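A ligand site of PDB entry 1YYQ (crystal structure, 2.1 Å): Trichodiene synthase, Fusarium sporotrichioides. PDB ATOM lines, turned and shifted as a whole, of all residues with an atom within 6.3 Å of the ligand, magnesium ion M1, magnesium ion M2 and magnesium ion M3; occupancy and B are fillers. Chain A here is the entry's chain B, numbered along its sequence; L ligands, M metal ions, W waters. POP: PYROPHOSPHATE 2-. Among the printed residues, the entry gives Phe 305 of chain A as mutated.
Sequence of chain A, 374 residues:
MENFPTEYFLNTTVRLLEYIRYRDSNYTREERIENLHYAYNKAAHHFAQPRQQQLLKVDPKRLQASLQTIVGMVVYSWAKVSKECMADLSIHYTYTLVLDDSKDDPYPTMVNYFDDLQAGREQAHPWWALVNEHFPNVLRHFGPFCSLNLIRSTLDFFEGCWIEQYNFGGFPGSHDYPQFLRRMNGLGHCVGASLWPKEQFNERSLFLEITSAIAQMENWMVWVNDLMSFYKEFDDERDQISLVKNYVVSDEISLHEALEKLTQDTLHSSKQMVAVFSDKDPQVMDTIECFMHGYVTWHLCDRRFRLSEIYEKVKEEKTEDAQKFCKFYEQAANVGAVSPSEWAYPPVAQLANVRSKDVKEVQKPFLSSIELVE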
ATOM      1  N   LEU A  97      -9.342 -37.482 -16.020  1.00  0.00           N
ATOM      2  CA  LEU A  97      -9.694 -36.749 -14.816  1.00  0.00           C
ATOM      3  C   LEU A  97      -8.820 -37.206 -13.647  1.00  0.00           C
ATOM      4  O   LEU A  97      -8.372 -36.389 -12.844  1.00  0.00           O
ATOM      5  CB  LEU A  97     -11.166 -36.944 -14.434  1.00  0.00           C
ATOM      6  CG  LEU A  97     -11.685 -35.865 -13.474  1.00  0.00           C
ATOM      7  CD1 LEU A  97     -11.758 -34.555 -14.230  1.00  0.00           C
ATOM      8  CD2 LEU A  97     -13.059 -36.220 -12.928  1.00  0.00           C
ATOM      9  N   ASP A 100      -5.673 -35.677 -13.987  1.00  0.00           N
ATOM     10  CA  ASP A 100      -5.885 -34.242 -13.807  1.00  0.00           C
ATOM     11  C   ASP A 100      -5.708 -33.701 -12.393  1.00  0.00           C
ATOM     12  O   ASP A 100      -5.322 -32.554 -12.202  1.00  0.00           O
ATOM     13  CB  ASP A 100      -7.275 -33.857 -14.329  1.00  0.00           C
ATOM     14  CG  ASP A 100      -7.494 -32.365 -14.353  1.00  0.00           C
ATOM     15  OD1 ASP A 100      -8.160 -31.839 -13.419  1.00  0.00           O
ATOM     16  OD2 ASP A 100      -6.994 -31.703 -15.293  1.00  0.00           O
ATOM     17  N   ASP A 101      -6.005 -34.541 -11.393  1.00  0.00           N
ATOM     18  CA  ASP A 101      -5.879 -34.132 -10.002  1.00  0.00           C
ATOM     19  C   ASP A 101      -4.675 -34.773  -9.321  1.00  0.00           C
ATOM     20  O   ASP A 101      -4.424 -34.545  -8.134  1.00  0.00           O
ATOM     21  CB  ASP A 101      -7.133 -34.526  -9.198  1.00  0.00           C
ATOM     22  CG  ASP A 101      -8.394 -33.885  -9.716  1.00  0.00           C
ATOM     23  OD1 ASP A 101      -8.382 -32.675 -10.063  1.00  0.00           O
ATOM     24  OD2 ASP A 101      -9.419 -34.599  -9.760  1.00  0.00           O
ATOM     25  N   PHE A 157      -2.395 -33.305 -23.215  1.00  0.00           N
ATOM     26  CA  PHE A 157      -2.902 -33.295 -21.853  1.00  0.00           C
ATOM     27  C   PHE A 157      -1.882 -33.908 -20.905  1.00  0.00           C
ATOM     28  O   PHE A 157      -1.634 -33.367 -19.825  1.00  0.00           O
ATOM     29  CB  PHE A 157      -4.211 -34.097 -21.791  1.00  0.00           C
ATOM     30  CG  PHE A 157      -4.769 -34.226 -20.403  1.00  0.00           C
ATOM     31  CD1 PHE A 157      -5.309 -33.128 -19.754  1.00  0.00           C
ATOM     32  CD2 PHE A 157      -4.737 -35.447 -19.743  1.00  0.00           C
ATOM     33  CE1 PHE A 157      -5.797 -33.243 -18.455  1.00  0.00           C
ATOM     34  CE2 PHE A 157      -5.218 -35.569 -18.445  1.00  0.00           C
ATOM     35  CZ  PHE A 157      -5.751 -34.463 -17.805  1.00  0.00           C
ATOM     36  N   CYS A 161      -0.246 -31.951 -17.658  1.00  0.00           N
ATOM     37  CA  CYS A 161      -0.277 -32.368 -16.259  1.00  0.00           C
ATOM     38  C   CYS A 161       1.158 -32.481 -15.730  1.00  0.00           C
ATOM     39  O   CYS A 161       1.395 -32.328 -14.526  1.00  0.00           O
ATOM     40  CB  CYS A 161      -0.982 -33.720 -16.120  1.00  0.00           C
ATOM     41  SG  CYS A 161      -2.765 -33.679 -16.500  1.00  0.00           S
ATOM     42  N   GLU A 164       2.283 -28.842 -14.931  1.00  0.00           N
ATOM     43  CA  GLU A 164       1.610 -28.403 -13.707  1.00  0.00           C
ATOM     44  C   GLU A 164       2.272 -28.933 -12.439  1.00  0.00           C
ATOM     45  O   GLU A 164       2.137 -28.329 -11.369  1.00  0.00           O
ATOM     46  CB  GLU A 164       0.142 -28.824 -13.721  1.00  0.00           C
ATOM     47  CG  GLU A 164      -0.666 -28.209 -14.852  1.00  0.00           C
ATOM     48  CD  GLU A 164      -2.120 -28.659 -14.870  1.00  0.00           C
ATOM     49  OE1 GLU A 164      -2.420 -29.778 -14.406  1.00  0.00           O
ATOM     50  OE2 GLU A 164      -2.962 -27.877 -15.353  1.00  0.00           O
ATOM     51  N   ARG A 182      -2.880 -23.708 -21.009  1.00  0.00           N
ATOM     52  CA  ARG A 182      -4.297 -24.018 -21.044  1.00  0.00           C
ATOM     53  C   ARG A 182      -4.640 -24.903 -22.244  1.00  0.00           C
ATOM     54  O   ARG A 182      -5.391 -25.874 -22.110  1.00  0.00           O
ATOM     55  CB  ARG A 182      -5.140 -22.736 -21.063  1.00  0.00           C
ATOM     56  CG  ARG A 182      -6.649 -22.977 -20.873  1.00  0.00           C
ATOM     57  CD  ARG A 182      -6.884 -24.012 -19.785  1.00  0.00           C
ATOM     58  NE  ARG A 182      -8.298 -24.107 -19.406  1.00  0.00           N
ATOM     59  CZ  ARG A 182      -8.816 -25.104 -18.687  1.00  0.00           C
ATOM     60  NH1 ARG A 182      -8.033 -26.101 -18.283  1.00  0.00           N
ATOM     61  NH2 ARG A 182     -10.103 -25.101 -18.383  1.00  0.00           N
ATOM     62  N   ASN A 185      -3.266 -28.477 -21.468  1.00  0.00           N
ATOM     63  CA  ASN A 185      -4.043 -29.312 -20.548  1.00  0.00           C
ATOM     64  C   ASN A 185      -5.543 -29.296 -20.800  1.00  0.00           C
ATOM     65  O   ASN A 185      -6.304 -29.939 -20.080  1.00  0.00           O
ATOM     66  CB  ASN A 185      -3.818 -28.840 -19.115  1.00  0.00           C
ATOM     67  CG  ASN A 185      -4.348 -27.435 -18.870  1.00  0.00           C
ATOM     68  OD1 ASN A 185      -5.399 -27.037 -19.400  1.00  0.00           O
ATOM     69  ND2 ASN A 185      -3.626 -26.657 -18.063  1.00  0.00           N
ATOM     70  N   GLY A 186      -5.968 -28.573 -21.831  1.00  0.00           N
ATOM     71  CA  GLY A 186      -7.382 -28.454 -22.105  1.00  0.00           C
ATOM     72  C   GLY A 186      -8.164 -29.598 -22.701  1.00  0.00           C
ATOM     73  O   GLY A 186      -9.388 -29.614 -22.583  1.00  0.00           O
ATOM     74  N   VAL A 222     -12.658 -24.760 -22.862  1.00  0.00           N
ATOM     75  CA  VAL A 222     -11.714 -24.551 -21.769  1.00  0.00           C
ATOM     76  C   VAL A 222     -12.040 -23.315 -20.934  1.00  0.00           C
ATOM     77  O   VAL A 222     -12.018 -23.352 -19.702  1.00  0.00           O
ATOM     78  CB  VAL A 222     -10.250 -24.439 -22.287  1.00  0.00           C
ATOM     79  CG1 VAL A 222      -9.825 -25.753 -22.923  1.00  0.00           C
ATOM     80  CG2 VAL A 222     -10.120 -23.295 -23.295  1.00  0.00           C
ATOM     81  N   ASN A 225     -14.961 -23.652 -18.557  1.00  0.00           N
ATOM     82  CA  ASN A 225     -14.585 -24.383 -17.355  1.00  0.00           C
ATOM     83  C   ASN A 225     -13.712 -23.516 -16.452  1.00  0.00           C
ATOM     84  O   ASN A 225     -13.811 -23.599 -15.228  1.00  0.00           O
ATOM     85  CB  ASN A 225     -13.848 -25.679 -17.703  1.00  0.00           C
ATOM     86  CG  ASN A 225     -13.252 -26.352 -16.471  1.00  0.00           C
ATOM     87  OD1 ASN A 225     -12.131 -26.046 -16.072  1.00  0.00           O
ATOM     88  ND2 ASN A 225     -14.009 -27.255 -15.868  1.00  0.00           N
ATOM     89  N   ASP A 226     -12.857 -22.688 -17.048  1.00  0.00           N
ATOM     90  CA  ASP A 226     -12.020 -21.827 -16.227  1.00  0.00           C
ATOM     91  C   ASP A 226     -12.894 -20.928 -15.370  1.00  0.00           C
ATOM     92  O   ASP A 226     -12.615 -20.698 -14.192  1.00  0.00           O
ATOM     93  CB  ASP A 226     -11.087 -20.985 -17.115  1.00  0.00           C
ATOM     94  CG  ASP A 226      -9.864 -21.762 -17.585  1.00  0.00           C
ATOM     95  OD1 ASP A 226      -9.262 -22.473 -16.755  1.00  0.00           O
ATOM     96  OD2 ASP A 226      -9.504 -21.664 -18.776  1.00  0.00           O
ATOM     97  N   SER A 229     -15.411 -23.425 -13.056  1.00  0.00           N
ATOM     98  CA  SER A 229     -14.646 -24.160 -12.058  1.00  0.00           C
ATOM     99  C   SER A 229     -13.759 -23.224 -11.224  1.00  0.00           C
ATOM    100  O   SER A 229     -12.957 -23.689 -10.411  1.00  0.00           O
ATOM    101  CB  SER A 229     -13.759 -25.223 -12.720  1.00  0.00           C
ATOM    102  OG  SER A 229     -12.609 -24.657 -13.311  1.00  0.00           O
ATOM    103  N   PHE A 230     -13.917 -21.922 -11.433  1.00  0.00           N
ATOM    104  CA  PHE A 230     -13.115 -20.955 -10.684  1.00  0.00           C
ATOM    105  C   PHE A 230     -13.347 -21.077  -9.193  1.00  0.00           C
ATOM    106  O   PHE A 230     -12.487 -20.715  -8.399  1.00  0.00           O
ATOM    107  CB  PHE A 230     -13.448 -19.531 -11.136  1.00  0.00           C
ATOM    108  CG  PHE A 230     -12.666 -18.470 -10.392  1.00  0.00           C
ATOM    109  CD1 PHE A 230     -11.273 -18.492 -10.385  1.00  0.00           C
ATOM    110  CD2 PHE A 230     -13.327 -17.456  -9.707  1.00  0.00           C
ATOM    111  CE1 PHE A 230     -10.542 -17.512  -9.706  1.00  0.00           C
ATOM    112  CE2 PHE A 230     -12.610 -16.476  -9.028  1.00  0.00           C
ATOM    113  CZ  PHE A 230     -11.217 -16.498  -9.021  1.00  0.00           C
ATOM    114  N   LYS A 232     -14.272 -24.151  -7.285  1.00  0.00           N
ATOM    115  CA  LYS A 232     -13.654 -25.344  -6.701  1.00  0.00           C
ATOM    116  C   LYS A 232     -12.146 -25.174  -6.732  1.00  0.00           C
ATOM    117  O   LYS A 232     -11.421 -25.658  -5.852  1.00  0.00           O
ATOM    118  CB  LYS A 232     -14.084 -26.624  -7.443  1.00  0.00           C
ATOM    119  CG  LYS A 232     -13.494 -26.834  -8.819  1.00  0.00           C
ATOM    120  CD  LYS A 232     -12.193 -27.640  -8.757  1.00  0.00           C
ATOM    121  CE  LYS A 232     -11.740 -28.082 -10.154  1.00  0.00           C
ATOM    122  NZ  LYS A 232     -10.511 -28.937 -10.140  1.00  0.00           N
ATOM    123  N   GLU A 233     -11.667 -24.489  -7.759  1.00  0.00           N
ATOM    124  CA  GLU A 233     -10.250 -24.177  -7.897  1.00  0.00           C
ATOM    125  C   GLU A 233     -10.187 -22.847  -7.177  1.00  0.00           C
ATOM    126  O   GLU A 233     -11.169 -22.102  -7.189  1.00  0.00           O
ATOM    127  CB  GLU A 233      -9.875 -23.973  -9.374  1.00  0.00           C
ATOM    128  CG  GLU A 233     -10.135 -25.172 -10.263  1.00  0.00           C
ATOM    129  CD  GLU A 233      -9.788 -24.927 -11.723  1.00  0.00           C
ATOM    130  OE1 GLU A 233      -9.742 -25.912 -12.494  1.00  0.00           O
ATOM    131  OE2 GLU A 233      -9.551 -23.758 -12.097  1.00  0.00           O
ATOM    132  N   ARG A 238      -3.698 -28.522  -5.670  1.00  0.00           N
ATOM    133  CA  ARG A 238      -3.394 -29.100  -6.979  1.00  0.00           C
ATOM    134  C   ARG A 238      -3.676 -28.119  -8.096  1.00  0.00           C
ATOM    135  O   ARG A 238      -3.049 -28.176  -9.162  1.00  0.00           O
ATOM    136  CB  ARG A 238      -4.220 -30.374  -7.242  1.00  0.00           C
ATOM    137  CG  ARG A 238      -4.057 -30.930  -8.669  1.00  0.00           C
ATOM    138  CD  ARG A 238      -2.590 -31.281  -8.964  1.00  0.00           C
ATOM    139  NE  ARG A 238      -2.357 -31.855 -10.292  1.00  0.00           N
ATOM    140  CZ  ARG A 238      -2.380 -31.179 -11.443  1.00  0.00           C
ATOM    141  NH1 ARG A 238      -2.644 -29.876 -11.449  1.00  0.00           N
ATOM    142  NH2 ARG A 238      -2.126 -31.809 -12.579  1.00  0.00           N
ATOM    143  N   ASP A 239      -4.636 -27.236  -7.881  1.00  0.00           N
ATOM    144  CA  ASP A 239      -4.946 -26.260  -8.888  1.00  0.00           C
ATOM    145  C   ASP A 239      -4.029 -25.065  -8.628  1.00  0.00           C
ATOM    146  O   ASP A 239      -2.808 -25.239  -8.648  1.00  0.00           O
ATOM    147  CB  ASP A 239      -6.449 -25.916  -8.839  1.00  0.00           C
ATOM    148  CG  ASP A 239      -7.331 -27.149  -9.086  1.00  0.00           C
ATOM    149  OD1 ASP A 239      -6.783 -28.217  -9.455  1.00  0.00           O
ATOM    150  OD2 ASP A 239      -8.568 -27.075  -8.910  1.00  0.00           O
ATOM    151  N   TRP A 298     -23.811 -29.430 -16.546  1.00  0.00           N
ATOM    152  CA  TRP A 298     -22.870 -30.272 -15.810  1.00  0.00           C
ATOM    153  C   TRP A 298     -22.069 -29.487 -14.759  1.00  0.00           C
ATOM    154  O   TRP A 298     -21.917 -29.932 -13.618  1.00  0.00           O
ATOM    155  CB  TRP A 298     -21.931 -30.954 -16.802  1.00  0.00           C
ATOM    156  CG  TRP A 298     -20.841 -31.730 -16.165  1.00  0.00           C
ATOM    157  CD1 TRP A 298     -20.978 -32.843 -15.375  1.00  0.00           C
ATOM    158  CD2 TRP A 298     -19.439 -31.480 -16.274  1.00  0.00           C
ATOM    159  NE1 TRP A 298     -19.737 -33.294 -14.997  1.00  0.00           N
ATOM    160  CE2 TRP A 298     -18.776 -32.471 -15.533  1.00  0.00           C
ATOM    161  CE3 TRP A 298     -18.674 -30.504 -16.935  1.00  0.00           C
ATOM    162  CZ2 TRP A 298     -17.376 -32.533 -15.421  1.00  0.00           C
ATOM    163  CZ3 TRP A 298     -17.288 -30.550 -16.831  1.00  0.00           C
ATOM    164  CH2 TRP A 298     -16.646 -31.563 -16.084  1.00  0.00           C
ATOM    165  N   HIS A 299     -21.543 -28.325 -15.154  1.00  0.00           N
ATOM    166  CA  HIS A 299     -20.770 -27.503 -14.228  1.00  0.00           C
ATOM    167  C   HIS A 299     -21.626 -27.027 -13.049  1.00  0.00           C
ATOM    168  O   HIS A 299     -21.143 -26.958 -11.910  1.00  0.00           O
ATOM    169  CB  HIS A 299     -20.179 -26.304 -14.963  1.00  0.00           C
ATOM    170  CG  HIS A 299     -19.003 -26.632 -15.821  1.00  0.00           C
ATOM    171  ND1 HIS A 299     -17.738 -26.814 -15.305  1.00  0.00           N
ATOM    172  CD2 HIS A 299     -18.900 -26.853 -17.149  1.00  0.00           C
ATOM    173  CE1 HIS A 299     -16.908 -27.123 -16.292  1.00  0.00           C
ATOM    174  NE2 HIS A 299     -17.596 -27.155 -17.425  1.00  0.00           N
ATOM    175  N   ARG A 304     -18.168 -32.037  -8.198  1.00  0.00           N
ATOM    176  CA  ARG A 304     -16.785 -31.605  -8.406  1.00  0.00           C
ATOM    177  C   ARG A 304     -16.601 -30.094  -8.355  1.00  0.00           C
ATOM    178  O   ARG A 304     -15.591 -29.603  -7.853  1.00  0.00           O
ATOM    179  CB  ARG A 304     -16.240 -32.122  -9.745  1.00  0.00           C
ATOM    180  CG  ARG A 304     -14.773 -31.752 -10.015  1.00  0.00           C
ATOM    181  CD  ARG A 304     -14.347 -32.090 -11.434  1.00  0.00           C
ATOM    182  NE  ARG A 304     -12.951 -31.757 -11.731  1.00  0.00           N
ATOM    183  CZ  ARG A 304     -11.896 -32.425 -11.258  1.00  0.00           C
ATOM    184  NH1 ARG A 304     -12.061 -33.456 -10.444  1.00  0.00           N
ATOM    185  NH2 ARG A 304     -10.670 -32.052 -11.609  1.00  0.00           N
ATOM    186  N   PHE A 305     -17.570 -29.350  -8.855  1.00  0.00           N
ATOM    187  CA  PHE A 305     -17.457 -27.896  -8.885  1.00  0.00           C
ATOM    188  C   PHE A 305     -18.121 -27.183  -7.715  1.00  0.00           C
ATOM    189  O   PHE A 305     -18.052 -25.956  -7.592  1.00  0.00           O
ATOM    190  CB  PHE A 305     -17.984 -27.394 -10.208  1.00  0.00           C
ATOM    191  CG  PHE A 305     -17.349 -28.078 -11.384  1.00  0.00           C
ATOM    192  CD1 PHE A 305     -18.073 -28.958 -12.177  1.00  0.00           C
ATOM    193  CD2 PHE A 305     -15.997 -27.877 -11.663  1.00  0.00           C
ATOM    194  CE1 PHE A 305     -17.458 -29.642 -13.231  1.00  0.00           C
ATOM    195  CE2 PHE A 305     -15.375 -28.553 -12.715  1.00  0.00           C
ATOM    196  CZ  PHE A 305     -16.113 -29.436 -13.499  1.00  0.00           C
HETATM  197  P1  POP L   1      -9.262 -28.511 -15.720  1.00  0.00           P
HETATM  198  O1  POP L   1      -9.403 -27.014 -15.489  1.00  0.00           O
HETATM  199  O2  POP L   1      -8.028 -28.994 -15.043  1.00  0.00           O
HETATM  200  O3  POP L   1      -9.204 -28.854 -17.171  1.00  0.00           O
HETATM  201  O   POP L   1     -10.703 -29.178 -15.319  1.00  0.00           O
HETATM  202  P2  POP L   1     -11.394 -29.090 -13.812  1.00  0.00           P
HETATM  203  O4  POP L   1     -11.733 -27.608 -13.482  1.00  0.00           O
HETATM  204  O5  POP L   1     -10.351 -29.669 -12.857  1.00  0.00           O
HETATM  205  O6  POP L   1     -12.603 -29.867 -13.979  1.00  0.00           O
HETATM  206 MG    MG M   1     -10.727 -25.880 -14.387  1.00  0.00          MG
HETATM  207 MG    MG M   2      -8.076 -29.763 -13.025  1.00  0.00          MG
HETATM  208 MG    MG M   3      -6.270 -29.899 -15.464  1.00  0.00          MG
HETATM  209  O   HOH W   1      -7.023 -25.912 -14.990  1.00  0.00           O
HETATM  210  O   HOH W   2      -4.439 -30.604 -15.973  1.00  0.00           O
HETATM  211  O   HOH W   3      -5.887 -30.104 -13.246  1.00  0.00           O
HETATM  212  O   HOH W   4      -7.859 -30.261 -11.132  1.00  0.00           O
HETATM  213  O   HOH W   5      -7.986 -27.870 -12.196  1.00  0.00           O
HETATM  214  O   HOH W   6      -5.565 -27.988 -15.475  1.00  0.00           O
HETATM  215  O   HOH W   7      -9.994 -23.888 -14.780  1.00  0.00           O
HETATM  216  O   HOH W   8      -6.817 -29.957 -17.444  1.00  0.00           O
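Magnesium ion M3 is bound by OD2 of Asp 100 (2.0 Å). Magnesium ion M3 is bound by O2 of the ligand (2.0 Å). Magnesium ion M3 is bound by water W2, 2.0 Å away. Magnesium ion M3 is bound by water W6 (2.0 Å). Water W8 is bound to magnesium ion M3. Magnesium ion M3 is bound by water W3.
Magnesium ion M1 is bound by O1 of the ligand (2.1 Å), OE1 of Glu 233 (2.1 Å), water W7 (2.2 Å), O4 of the ligand (2.2 Å), OD1 of Asn 225 (2.2 Å) and OG of Ser 229 (2.5 Å).
Magnesium ion M2 is bound by water W4 (2.0 Å), water W5 (2.1 Å), OD1 of Asp 100 (2.1 Å), O2 of the ligand (2.2 Å), water W3 (2.2 Å) and O5 of the ligand (2.3 Å).
Merely in contact with magnesium ion M2: Lys 232 and Arg 304.
Of the 22 residues printed, 3 come within 4 Å of magnesium ion M1. The nearest printed residue that does not touch magnesium ion M1 is Arg 182 (4.1 Å).
OD1 of Asp 100 lies close to NH2 of Arg 304, at 3.1 Å. The side-chain amide nitrogen (ND2) of Asn 185 is in hydrogen-bond range of the side-chain carboxylate (OE2) of Glu 164, 3.0 Å away. O of Arg 182 sits close to OD1 of Asn 185 (2.9 Å). The side-chain carboxylate (OE1) of Glu 164 is in salt-bridge range of the guanidinium group (NH2) of Arg 238, 2.7 Å away. The backbone carbonyl oxygen of Asp 100 lies within hydrogen-bond range of the guanidinium group of Arg 238, at 3.3 Å. The side-chain amide oxygen (OD1) of Asn 225 lies close to the guanidinium group (NH2) of Arg 182 (3.2 Å). NZ of Lys 232 lies close to OE1 of Glu 233, at 3.9 Å. The guanidinium group (NH2) of Arg 304 is in salt-bridge range of the side-chain carboxylate (OD1) of Asp 101 (2.8 Å).
Glu 164 touches magnesium ion M3 (OE2 to MG, 3.9 Å).
NH1 of Arg 182 lies within salt-bridge range of O3 of the ligand, at 3.2 Å. The side-chain amino group of Lys 232 sits close to an oxygen (O5) of the ligand, at 2.8 Å. O6 of the ligand is in salt-bridge range of NE of Arg 304 (3.0 Å).
Water W7 bridges the side-chain carboxylate (OD1) of Asp 226 (2.5 Å) and the side-chain carboxylate (OE2) of Glu 233 (2.7 Å). Water W5 lies within hydrogen-bond range of OD1 of Asp 239 and NZ of Lys 232. Water W4 lies within hydrogen-bond range of the side-chain carboxylate (OD1) of Asp 101 (2.7 Å), the side-chain carboxylate (OD1) of Asp 239 (2.9 Å), the side-chain amino group (NZ) of Lys 232 (3.1 Å) and the guanidinium group (NH2) of Arg 304 (3.4 Å). Water W6 lies within hydrogen-bond range of the side-chain carboxylate (OE2) of Glu 164 and the side-chain amide nitrogen (ND2) of Asn 185. Water W8 lies within hydrogen-bond range of an oxygen (O3) of the ligand and the backbone carbonyl oxygen of Asn 185. Water W2 bridges the side-chain carboxylate (OE1) of Glu 164 (2.7 Å) and the side-chain sulfur (SG) of Cys 161 (3.5 Å).
Phe 305 touches the ligand. Hydrophobic or aromatic side chains that line the ligand: Phe 305. The nearest printed residue that does not touch the ligand is Asn 185 (4.2 Å).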
